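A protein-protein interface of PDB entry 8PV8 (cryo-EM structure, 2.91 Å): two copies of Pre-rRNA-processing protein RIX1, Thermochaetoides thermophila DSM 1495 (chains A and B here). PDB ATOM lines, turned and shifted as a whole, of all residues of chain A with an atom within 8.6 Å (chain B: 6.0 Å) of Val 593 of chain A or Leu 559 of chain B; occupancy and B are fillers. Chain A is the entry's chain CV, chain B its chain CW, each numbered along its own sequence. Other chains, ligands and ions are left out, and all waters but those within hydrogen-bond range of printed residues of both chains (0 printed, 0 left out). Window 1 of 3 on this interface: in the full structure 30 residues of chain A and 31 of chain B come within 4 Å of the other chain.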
ATOM      1  N   LEU A 559      17.089  -7.662 -11.965  1.00  0.00           N
ATOM      2  CA  LEU A 559      17.627  -8.178 -10.709  1.00  0.00           C
ATOM      3  C   LEU A 559      16.921  -9.454 -10.269  1.00  0.00           C
ATOM      4  O   LEU A 559      17.578 -10.395  -9.808  1.00  0.00           O
ATOM      5  CB  LEU A 559      17.536  -7.098  -9.624  1.00  0.00           C
ATOM      6  CG  LEU A 559      18.061  -7.360  -8.208  1.00  0.00           C
ATOM      7  CD1 LEU A 559      18.649  -6.101  -7.638  1.00  0.00           C
ATOM      8  CD2 LEU A 559      16.928  -7.800  -7.293  1.00  0.00           C
ATOM      9  N   LEU A 563      18.574 -13.148  -9.740  1.00  0.00           N
ATOM     10  CA  LEU A 563      18.515 -13.814  -8.445  1.00  0.00           C
ATOM     11  C   LEU A 563      17.597 -15.029  -8.422  1.00  0.00           C
ATOM     12  O   LEU A 563      17.618 -15.779  -7.442  1.00  0.00           O
ATOM     13  CB  LEU A 563      18.081 -12.823  -7.367  1.00  0.00           C
ATOM     14  CG  LEU A 563      19.048 -11.656  -7.191  1.00  0.00           C
ATOM     15  CD1 LEU A 563      18.620 -10.810  -6.021  1.00  0.00           C
ATOM     16  CD2 LEU A 563      20.475 -12.155  -7.034  1.00  0.00           C
ATOM     17  N   PRO A 586      24.406   1.281 -14.405  1.00  0.00           N
ATOM     18  CA  PRO A 586      25.715   0.894 -13.858  1.00  0.00           C
ATOM     19  C   PRO A 586      25.931   1.292 -12.409  1.00  0.00           C
ATOM     20  O   PRO A 586      26.694   0.640 -11.691  1.00  0.00           O
ATOM     21  CB  PRO A 586      26.699   1.623 -14.780  1.00  0.00           C
ATOM     22  CG  PRO A 586      25.950   2.821 -15.241  1.00  0.00           C
ATOM     23  CD  PRO A 586      24.505   2.417 -15.336  1.00  0.00           C
ATOM     24  N   ARG A 587      25.274   2.356 -11.968  1.00  0.00           N
ATOM     25  CA  ARG A 587      25.527   2.967 -10.671  1.00  0.00           C
ATOM     26  C   ARG A 587      24.259   2.998  -9.827  1.00  0.00           C
ATOM     27  O   ARG A 587      24.103   3.820  -8.920  1.00  0.00           O
ATOM     28  CB  ARG A 587      26.124   4.356 -10.869  1.00  0.00           C
ATOM     29  CG  ARG A 587      25.185   5.373 -11.501  1.00  0.00           C
ATOM     30  CD  ARG A 587      25.899   6.687 -11.749  1.00  0.00           C
ATOM     31  NE  ARG A 587      26.942   6.514 -12.753  1.00  0.00           N
ATOM     32  CZ  ARG A 587      28.244   6.530 -12.503  1.00  0.00           C
ATOM     33  NH1 ARG A 587      28.710   6.747 -11.285  1.00  0.00           N
ATOM     34  NH2 ARG A 587      29.098   6.310 -13.498  1.00  0.00           N
ATOM     35  N   ASP A 588      23.354   2.070 -10.101  1.00  0.00           N
ATOM     36  CA  ASP A 588      22.093   1.945  -9.391  1.00  0.00           C
ATOM     37  C   ASP A 588      22.284   1.074  -8.154  1.00  0.00           C
ATOM     38  O   ASP A 588      23.262   0.330  -8.031  1.00  0.00           O
ATOM     39  CB  ASP A 588      21.023   1.347 -10.316  1.00  0.00           C
ATOM     40  CG  ASP A 588      19.621   1.457  -9.750  1.00  0.00           C
ATOM     41  OD1 ASP A 588      18.829   0.507  -9.926  1.00  0.00           O
ATOM     42  OD2 ASP A 588      19.310   2.495  -9.128  1.00  0.00           O
ATOM     43  N   GLU A 589      21.331   1.188  -7.222  1.00  0.00           N
ATOM     44  CA  GLU A 589      21.354   0.364  -6.016  1.00  0.00           C
ATOM     45  C   GLU A 589      21.216  -1.117  -6.347  1.00  0.00           C
ATOM     46  O   GLU A 589      21.711  -1.971  -5.601  1.00  0.00           O
ATOM     47  CB  GLU A 589      20.253   0.819  -5.055  1.00  0.00           C
ATOM     48  CG  GLU A 589      18.831   0.778  -5.618  1.00  0.00           C
ATOM     49  CD  GLU A 589      18.144  -0.563  -5.420  1.00  0.00           C
ATOM     50  OE1 GLU A 589      18.593  -1.341  -4.551  1.00  0.00           O
ATOM     51  OE2 GLU A 589      17.157  -0.837  -6.135  1.00  0.00           O
ATOM     52  N   SER A 590      20.571  -1.436  -7.474  1.00  0.00           N
ATOM     53  CA  SER A 590      20.366  -2.825  -7.879  1.00  0.00           C
ATOM     54  C   SER A 590      21.689  -3.548  -8.112  1.00  0.00           C
ATOM     55  O   SER A 590      21.869  -4.692  -7.681  1.00  0.00           O
ATOM     56  CB  SER A 590      19.501  -2.870  -9.139  1.00  0.00           C
ATOM     57  OG  SER A 590      18.297  -2.147  -8.958  1.00  0.00           O
ATOM     58  N   VAL A 591      22.630  -2.892  -8.791  1.00  0.00           N
ATOM     59  CA  VAL A 591      23.935  -3.505  -9.007  1.00  0.00           C
ATOM     60  C   VAL A 591      24.889  -3.191  -7.858  1.00  0.00           C
ATOM     61  O   VAL A 591      25.840  -3.947  -7.609  1.00  0.00           O
ATOM     62  CB  VAL A 591      24.510  -3.065 -10.362  1.00  0.00           C
ATOM     63  CG1 VAL A 591      23.682  -3.645 -11.494  1.00  0.00           C
ATOM     64  CG2 VAL A 591      24.523  -1.556 -10.459  1.00  0.00           C
ATOM     65  N   GLU A 592      24.655  -2.091  -7.135  1.00  0.00           N
ATOM     66  CA  GLU A 592      25.452  -1.791  -5.953  1.00  0.00           C
ATOM     67  C   GLU A 592      25.256  -2.817  -4.846  1.00  0.00           C
ATOM     68  O   GLU A 592      26.191  -3.059  -4.078  1.00  0.00           O
ATOM     69  CB  GLU A 592      25.118  -0.391  -5.442  1.00  0.00           C
ATOM     70  CG  GLU A 592      26.273   0.305  -4.744  1.00  0.00           C
ATOM     71  CD  GLU A 592      25.955   1.742  -4.380  1.00  0.00           C
ATOM     72  OE1 GLU A 592      24.771   2.130  -4.469  1.00  0.00           O
ATOM     73  OE2 GLU A 592      26.889   2.484  -4.008  1.00  0.00           O
ATOM     74  N   VAL A 593      24.072  -3.421  -4.749  1.00  0.00           N
ATOM     75  CA  VAL A 593      23.858  -4.559  -3.865  1.00  0.00           C
ATOM     76  C   VAL A 593      24.598  -5.808  -4.338  1.00  0.00           C
ATOM     77  O   VAL A 593      25.254  -6.471  -3.521  1.00  0.00           O
ATOM     78  CB  VAL A 593      22.348  -4.845  -3.713  1.00  0.00           C
ATOM     79  CG1 VAL A 593      22.105  -6.208  -3.093  1.00  0.00           C
ATOM     80  CG2 VAL A 593      21.701  -3.770  -2.863  1.00  0.00           C
ATOM     81  N   LEU A 594      24.547  -6.127  -5.631  1.00  0.00           N
ATOM     82  CA  LEU A 594      25.241  -7.293  -6.164  1.00  0.00           C
ATOM     83  C   LEU A 594      26.757  -7.153  -6.132  1.00  0.00           C
ATOM     84  O   LEU A 594      27.458  -8.162  -6.260  1.00  0.00           O
ATOM     85  CB  LEU A 594      24.775  -7.570  -7.594  1.00  0.00           C
ATOM     86  CG  LEU A 594      23.439  -8.306  -7.703  1.00  0.00           C
ATOM     87  CD1 LEU A 594      22.939  -8.314  -9.135  1.00  0.00           C
ATOM     88  CD2 LEU A 594      23.577  -9.722  -7.176  1.00  0.00           C
ATOM     89  N   ARG A 595      27.276  -5.939  -5.970  1.00  0.00           N
ATOM     90  CA  ARG A 595      28.705  -5.725  -5.778  1.00  0.00           C
ATOM     91  C   ARG A 595      29.118  -5.740  -4.309  1.00  0.00           C
ATOM     92  O   ARG A 595      30.090  -5.072  -3.945  1.00  0.00           O
ATOM     93  CB  ARG A 595      29.138  -4.405  -6.417  1.00  0.00           C
ATOM     94  CG  ARG A 595      29.179  -4.427  -7.928  1.00  0.00           C
ATOM     95  CD  ARG A 595      29.879  -3.194  -8.456  1.00  0.00           C
ATOM     96  NE  ARG A 595      28.950  -2.098  -8.694  1.00  0.00           N
ATOM     97  CZ  ARG A 595      28.558  -1.698  -9.896  1.00  0.00           C
ATOM     98  NH1 ARG A 595      28.974  -2.301 -10.996  1.00  0.00           N
ATOM     99  NH2 ARG A 595      27.733  -0.661  -9.995  1.00  0.00           N
ATOM    100  N   SER A 596      28.404  -6.479  -3.455  1.00  0.00           N
ATOM    101  CA  SER A 596      28.710  -6.468  -2.027  1.00  0.00           C
ATOM    102  C   SER A 596      29.855  -7.402  -1.659  1.00  0.00           C
ATOM    103  O   SER A 596      30.269  -7.420  -0.495  1.00  0.00           O
ATOM    104  CB  SER A 596      27.474  -6.845  -1.209  1.00  0.00           C
ATOM    105  OG  SER A 596      26.366  -6.033  -1.550  1.00  0.00           O
ATOM    106  N   ASN A 597      30.375  -8.175  -2.609  1.00  0.00           N
ATOM    107  CA  ASN A 597      31.465  -9.096  -2.308  1.00  0.00           C
ATOM    108  C   ASN A 597      32.810  -8.379  -2.304  1.00  0.00           C
ATOM    109  O   ASN A 597      33.842  -8.982  -1.994  1.00  0.00           O
ATOM    110  CB  ASN A 597      31.476 -10.255  -3.307  1.00  0.00           C
ATOM    111  CG  ASN A 597      31.397  -9.789  -4.747  1.00  0.00           C
ATOM    112  OD1 ASN A 597      31.265  -8.597  -5.022  1.00  0.00           O
ATOM    113  ND2 ASN A 597      31.475 -10.733  -5.677  1.00  0.00           N
ATOM    114  N   LEU A 598      32.809  -7.089  -2.648  1.00  0.00           N
ATOM    115  CA  LEU A 598      34.020  -6.286  -2.667  1.00  0.00           C
ATOM    116  C   LEU A 598      34.077  -5.249  -1.553  1.00  0.00           C
ATOM    117  O   LEU A 598      34.957  -4.383  -1.587  1.00  0.00           O
ATOM    118  CB  LEU A 598      34.160  -5.569  -4.018  1.00  0.00           C
ATOM    119  CG  LEU A 598      34.305  -6.446  -5.260  1.00  0.00           C
ATOM    120  CD1 LEU A 598      34.268  -5.590  -6.513  1.00  0.00           C
ATOM    121  CD2 LEU A 598      35.589  -7.255  -5.197  1.00  0.00           C
ATOM    122  N   VAL A 599      33.167  -5.308  -0.578  1.00  0.00           N
ATOM    123  CA  VAL A 599      33.040  -4.239   0.411  1.00  0.00           C
ATOM    124  C   VAL A 599      34.223  -4.217   1.372  1.00  0.00           C
ATOM    125  O   VAL A 599      34.760  -3.141   1.673  1.00  0.00           O
ATOM    126  CB  VAL A 599      31.695  -4.381   1.151  1.00  0.00           C
ATOM    127  CG1 VAL A 599      31.665  -3.533   2.413  1.00  0.00           C
ATOM    128  CG2 VAL A 599      30.549  -3.993   0.233  1.00  0.00           C
ATOM    129  N   ASN B 554      13.823   2.473   7.004  1.00  0.00           N
ATOM    130  CA  ASN B 554      14.127   2.829   5.626  1.00  0.00           C
ATOM    131  C   ASN B 554      15.068   1.781   5.047  1.00  0.00           C
ATOM    132  O   ASN B 554      16.263   1.765   5.370  1.00  0.00           O
ATOM    133  CB  ASN B 554      14.744   4.225   5.554  1.00  0.00           C
ATOM    134  CG  ASN B 554      14.799   4.773   4.141  1.00  0.00           C
ATOM    135  OD1 ASN B 554      14.370   4.124   3.188  1.00  0.00           O
ATOM    136  ND2 ASN B 554      15.324   5.984   4.002  1.00  0.00           N
ATOM    137  N   GLN B 555      14.522   0.917   4.185  1.00  0.00           N
ATOM    138  CA  GLN B 555      15.279  -0.217   3.664  1.00  0.00           C
ATOM    139  C   GLN B 555      16.445   0.236   2.796  1.00  0.00           C
ATOM    140  O   GLN B 555      17.544  -0.322   2.887  1.00  0.00           O
ATOM    141  CB  GLN B 555      14.352  -1.140   2.873  1.00  0.00           C
ATOM    142  CG  GLN B 555      15.047  -2.349   2.279  1.00  0.00           C
ATOM    143  CD  GLN B 555      14.245  -2.995   1.174  1.00  0.00           C
ATOM    144  OE1 GLN B 555      13.157  -2.535   0.829  1.00  0.00           O
ATOM    145  NE2 GLN B 555      14.782  -4.066   0.603  1.00  0.00           N
ATOM    146  N   SER B 556      16.227   1.252   1.957  1.00  0.00           N
ATOM    147  CA  SER B 556      17.308   1.777   1.126  1.00  0.00           C
ATOM    148  C   SER B 556      18.406   2.397   1.979  1.00  0.00           C
ATOM    149  O   SER B 556      19.595   2.257   1.669  1.00  0.00           O
ATOM    150  CB  SER B 556      16.757   2.799   0.135  1.00  0.00           C
ATOM    151  OG  SER B 556      15.661   2.265  -0.586  1.00  0.00           O
ATOM    152  N   ALA B 557      18.026   3.082   3.060  1.00  0.00           N
ATOM    153  CA  ALA B 557      19.016   3.673   3.952  1.00  0.00           C
ATOM    154  C   ALA B 557      19.843   2.607   4.662  1.00  0.00           C
ATOM    155  O   ALA B 557      21.064   2.752   4.789  1.00  0.00           O
ATOM    156  CB  ALA B 557      18.333   4.587   4.966  1.00  0.00           C
ATOM    157  N   MET B 558      19.205   1.525   5.125  1.00  0.00           N
ATOM    158  CA  MET B 558      19.978   0.451   5.751  1.00  0.00           C
ATOM    159  C   MET B 558      20.859  -0.274   4.739  1.00  0.00           C
ATOM    160  O   MET B 558      21.984  -0.673   5.066  1.00  0.00           O
ATOM    161  CB  MET B 558      19.067  -0.547   6.464  1.00  0.00           C
ATOM    162  CG  MET B 558      18.036   0.051   7.387  1.00  0.00           C
ATOM    163  SD  MET B 558      17.292  -1.222   8.419  1.00  0.00           S
ATOM    164  CE  MET B 558      15.592  -0.682   8.454  1.00  0.00           C
ATOM    165  N   LEU B 559      20.367  -0.453   3.506  1.00  0.00           N
ATOM    166  CA  LEU B 559      21.189  -1.028   2.445  1.00  0.00           C
ATOM    167  C   LEU B 559      22.421  -0.175   2.180  1.00  0.00           C
ATOM    168  O   LEU B 559      23.536  -0.698   2.071  1.00  0.00           O
ATOM    169  CB  LEU B 559      20.373  -1.167   1.159  1.00  0.00           C
ATOM    170  CG  LEU B 559      19.785  -2.503   0.702  1.00  0.00           C
ATOM    171  CD1 LEU B 559      18.830  -3.089   1.713  1.00  0.00           C
ATOM    172  CD2 LEU B 559      19.084  -2.312  -0.630  1.00  0.00           C
ATOM    173  N   ALA B 560      22.239   1.144   2.099  1.00  0.00           N
ATOM    174  CA  ALA B 560      23.360   2.042   1.852  1.00  0.00           C
ATOM    175  C   ALA B 560      24.330   2.062   3.027  1.00  0.00           C
ATOM    176  O   ALA B 560      25.550   2.111   2.833  1.00  0.00           O
ATOM    177  CB  ALA B 560      22.835   3.444   1.558  1.00  0.00           C
ATOM    178  N   SER B 561      23.804   2.009   4.254  1.00  0.00           N
ATOM    179  CA  SER B 561      24.659   2.006   5.437  1.00  0.00           C
ATOM    180  C   SER B 561      25.487   0.730   5.526  1.00  0.00           C
ATOM    181  O   SER B 561      26.655   0.768   5.926  1.00  0.00           O
ATOM    182  CB  SER B 561      23.810   2.182   6.694  1.00  0.00           C
ATOM    183  OG  SER B 561      24.618   2.183   7.857  1.00  0.00           O
ATOM    184  N   CYS B 562      24.899  -0.412   5.163  1.00  0.00           N
ATOM    185  CA  CYS B 562      25.659  -1.657   5.178  1.00  0.00           C
ATOM    186  C   CYS B 562      26.629  -1.730   4.005  1.00  0.00           C
ATOM    187  O   CYS B 562      27.684  -2.367   4.104  1.00  0.00           O
ATOM    188  CB  CYS B 562      24.711  -2.854   5.174  1.00  0.00           C
ATOM    189  SG  CYS B 562      23.671  -2.990   6.642  1.00  0.00           S
ATOM    190  N   LEU B 563      26.290  -1.089   2.884  1.00  0.00           N
ATOM    191  CA  LEU B 563      27.202  -1.075   1.743  1.00  0.00           C
ATOM    192  C   LEU B 563      28.380  -0.141   1.984  1.00  0.00           C
ATOM    193  O   LEU B 563      29.466  -0.349   1.434  1.00  0.00           O
ATOM    194  CB  LEU B 563      26.450  -0.674   0.477  1.00  0.00           C
ATOM    195  CG  LEU B 563      25.660  -1.786  -0.208  1.00  0.00           C
ATOM    196  CD1 LEU B 563      24.759  -1.217  -1.287  1.00  0.00           C
ATOM    197  CD2 LEU B 563      26.618  -2.805  -0.790  1.00  0.00           C
ATOM    198  N   HIS B 564      28.186   0.894   2.794  1.00  0.00           N
ATOM    199  CA  HIS B 564      29.257   1.838   3.085  1.00  0.00           C
ATOM    200  C   HIS B 564      29.569   1.823   4.573  1.00  0.00           C
ATOM    201  O   HIS B 564      28.954   2.584   5.337  1.00  0.00           O
ATOM    202  CB  HIS B 564      28.867   3.247   2.636  1.00  0.00           C
ATOM    203  CG  HIS B 564      28.474   3.335   1.194  1.00  0.00           C
ATOM    204  ND1 HIS B 564      27.226   2.968   0.739  1.00  0.00           N
ATOM    205  CD2 HIS B 564      29.166   3.744   0.105  1.00  0.00           C
ATOM    206  CE1 HIS B 564      27.165   3.148  -0.568  1.00  0.00           C
ATOM    207  NE2 HIS B 564      28.329   3.619  -0.978  1.00  0.00           N
ATOM    208  N   LEU B 581      18.466  -4.861   9.635  1.00  0.00           N
ATOM    209  CA  LEU B 581      17.947  -4.919   8.273  1.00  0.00           C
ATOM    210  C   LEU B 581      17.373  -6.287   7.933  1.00  0.00           C
ATOM    211  O   LEU B 581      16.273  -6.378   7.377  1.00  0.00           O
ATOM    212  CB  LEU B 581      19.057  -4.555   7.292  1.00  0.00           C
ATOM    213  CG  LEU B 581      18.751  -4.520   5.799  1.00  0.00           C
ATOM    214  CD1 LEU B 581      17.478  -3.747   5.500  1.00  0.00           C
ATOM    215  CD2 LEU B 581      19.934  -3.910   5.090  1.00  0.00           C
ATOM    216  N   GLU B 589      14.992  -9.278  -1.817  1.00  0.00           N
ATOM    217  CA  GLU B 589      16.055  -9.883  -2.608  1.00  0.00           C
ATOM    218  C   GLU B 589      17.382  -9.145  -2.504  1.00  0.00           C
ATOM    219  O   GLU B 589      18.432  -9.793  -2.543  1.00  0.00           O
ATOM    220  CB  GLU B 589      15.622  -9.975  -4.072  1.00  0.00           C
ATOM    221  CG  GLU B 589      14.462 -10.924  -4.294  1.00  0.00           C
ATOM    222  CD  GLU B 589      14.829 -12.369  -4.014  1.00  0.00           C
ATOM    223  OE1 GLU B 589      16.000 -12.746  -4.233  1.00  0.00           O
ATOM    224  OE2 GLU B 589      13.943 -13.130  -3.572  1.00  0.00           O
ATOM    225  N   SER B 590      17.366  -7.818  -2.388  1.00  0.00           N
ATOM    226  CA  SER B 590      18.594  -7.076  -2.136  1.00  0.00           C
ATOM    227  C   SER B 590      19.159  -7.372  -0.753  1.00  0.00           C
ATOM    228  O   SER B 590      20.379  -7.507  -0.595  1.00  0.00           O
ATOM    229  CB  SER B 590      18.344  -5.575  -2.292  1.00  0.00           C
ATOM    230  OG  SER B 590      17.173  -5.179  -1.601  1.00  0.00           O
ATOM    231  N   VAL B 591      18.280  -7.489   0.246  1.00  0.00           N
ATOM    232  CA  VAL B 591      18.703  -7.832   1.598  1.00  0.00           C
ATOM    233  C   VAL B 591      19.295  -9.234   1.638  1.00  0.00           C
ATOM    234  O   VAL B 591      20.258  -9.483   2.370  1.00  0.00           O
ATOM    235  CB  VAL B 591      17.523  -7.679   2.575  1.00  0.00           C
ATOM    236  CG1 VAL B 591      17.959  -7.943   4.007  1.00  0.00           C
ATOM    237  CG2 VAL B 591      16.931  -6.286   2.465  1.00  0.00           C
ATOM    238  N   VAL B 593      20.967 -10.801  -0.858  1.00  0.00           N
ATOM    239  CA  VAL B 593      22.306 -10.739  -1.444  1.00  0.00           C
ATOM    240  C   VAL B 593      23.274 -10.056  -0.487  1.00  0.00           C
ATOM    241  O   VAL B 593      24.419 -10.495  -0.312  1.00  0.00           O
ATOM    242  CB  VAL B 593      22.260 -10.025  -2.806  1.00  0.00           C
ATOM    243  CG1 VAL B 593      23.660  -9.813  -3.360  1.00  0.00           C
ATOM    244  CG2 VAL B 593      21.453 -10.834  -3.764  1.00  0.00           C
ATOM    245  N   LEU B 594      22.822  -8.971   0.147  1.00  0.00           N
ATOM    246  CA  LEU B 594      23.653  -8.259   1.110  1.00  0.00           C
ATOM    247  C   LEU B 594      24.019  -9.150   2.290  1.00  0.00           C
ATOM    248  O   LEU B 594      25.173  -9.173   2.732  1.00  0.00           O
ATOM    249  CB  LEU B 594      22.917  -7.005   1.575  1.00  0.00           C
ATOM    250  CG  LEU B 594      23.716  -5.894   2.241  1.00  0.00           C
ATOM    251  CD1 LEU B 594      24.544  -5.161   1.210  1.00  0.00           C
ATOM    252  CD2 LEU B 594      22.754  -4.944   2.910  1.00  0.00           C
ATOM    253  N   ASN B 597      26.540 -11.864   1.149  1.00  0.00           N
ATOM    254  CA  ASN B 597      27.838 -11.385   0.690  1.00  0.00           C
ATOM    255  C   ASN B 597      28.640 -10.669   1.772  1.00  0.00           C
ATOM    256  O   ASN B 597      29.857 -10.862   1.856  1.00  0.00           O
ATOM    257  CB  ASN B 597      27.649 -10.464  -0.520  1.00  0.00           C
ATOM    258  CG  ASN B 597      27.384 -11.234  -1.797  1.00  0.00           C
ATOM    259  OD1 ASN B 597      27.284 -12.460  -1.786  1.00  0.00           O
ATOM    260  ND2 ASN B 597      27.269 -10.517  -2.909  1.00  0.00           N
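The side-chain amide nitrogen (NE2) of Gln 555 of chain B is in hydrogen-bond range of the side-chain hydroxyl (OG) of Ser 590 of chain B (3.4 Å).
O of Ala 560 of chain B is in hydrogen-bond range of ND1 of His 564 of chain B (2.8 Å).
Among the printed residues, merely in contact across the chains: Leu 563 of chain A with Glu 589 of chain B (3.6 Å), Leu 563 of chain A with Val 593 of chain B (3.6 Å), Glu 592 of chain A with Leu 563 of chain B (3.3 Å), Glu 592 of chain A with His 564 of chain B (3.5 Å), Val 593 of chain A with Leu 559 of chain B (3.7 Å), Val 593 of chain A with Ser 590 of chain B (3.3 Å), Val 593 of chain A with Val 593 of chain B (3.7 Å), Leu 594 of chain A with Val 593 of chain B (3.8 Å), Ser 596 of chain A with Leu 563 of chain B (3.3 Å), Ser 596 of chain A with Leu 594 of chain B (3.4 Å), Ser 596 of chain A with Asn 597 of chain B (3.7 Å), Asn 597 of chain A with Asn 597 of chain B (3.9 Å) and Val 599 of chain A with Leu 563 of chain B (3.99 Å).
Val 593 of chain A touches just these residues of chain B: Leu 559, Ser 590 and Val 593.
Of chain A, only Val 593 comes within 4 Å of Leu 559 of chain B.
No residue of chain A comes within 4 Å of Ala 560 of chain B.
Printed residues of chain A within 4 Å of His 564 of chain B: Glu 592.
Of the printed residues of chain A, Leu 594 of chain B touches Ser 596.
Of the printed residues of chain A, Glu 589 of chain B touches Leu 563 (3.6 Å).
Arg 595 of chain A touches none of the printed residues of chain B.
Ser 561 of chain B touches none of the printed residues of chain A.
The nearest printed residue of chain A that does not touch Ser 590 of chain B is Glu 589 of chain A (4.8 Å).
Of the 16 printed residues of chain A, 7 touch a printed residue of chain B.
Printed residues of chain A that touch a printed residue of chain B: Leu 563, Glu 592, Val 593, Leu 594, Ser 596, Asn 597 and Val 599.
Hydrophobic or aromatic side chains of chain A that line the printed part of chain B: Leu 563, Val 593, Leu 594 and Val 599.
Printed residues of chain B that touch a printed residue of chain A: Leu 559, Leu 563, His 564, Glu 589, Ser 590, Val 593, Leu 594 and Asn 597.
Hydrophobic or aromatic side chains of chain B within 4 Å of the printed part of chain A: Leu 559, Leu 563, His 564, Val 593 and Leu 594.
Among the printed residues, 13 pairs touch across the chains.
Among the printed residues, no Asp or Glu carboxylate lies within 4 Å of a Lys or Arg side-chain nitrogen of the other chain.
Leu 563 of chain A touches Val 593 of chain B, but with the chains exchanged Val 593 of chain A does not touch Leu 563 of chain B (4.2 Å).
Val 593 of chain A touches Ser 590 of chain B, but with the chains exchanged Ser 590 of chain A does not touch Val 593 of chain B (6.9 Å).
Leu 594 of chain A touches Val 593 of chain B, but with the chains exchanged Val 593 of chain A does not touch Leu 594 of chain B (4.3 Å).
Asn 597 of chain A touches its own counterpart, Asn 597 of chain B.
Positions printed for both chains: 559, 563, 589, 590, 591, 593, 594 and 597.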
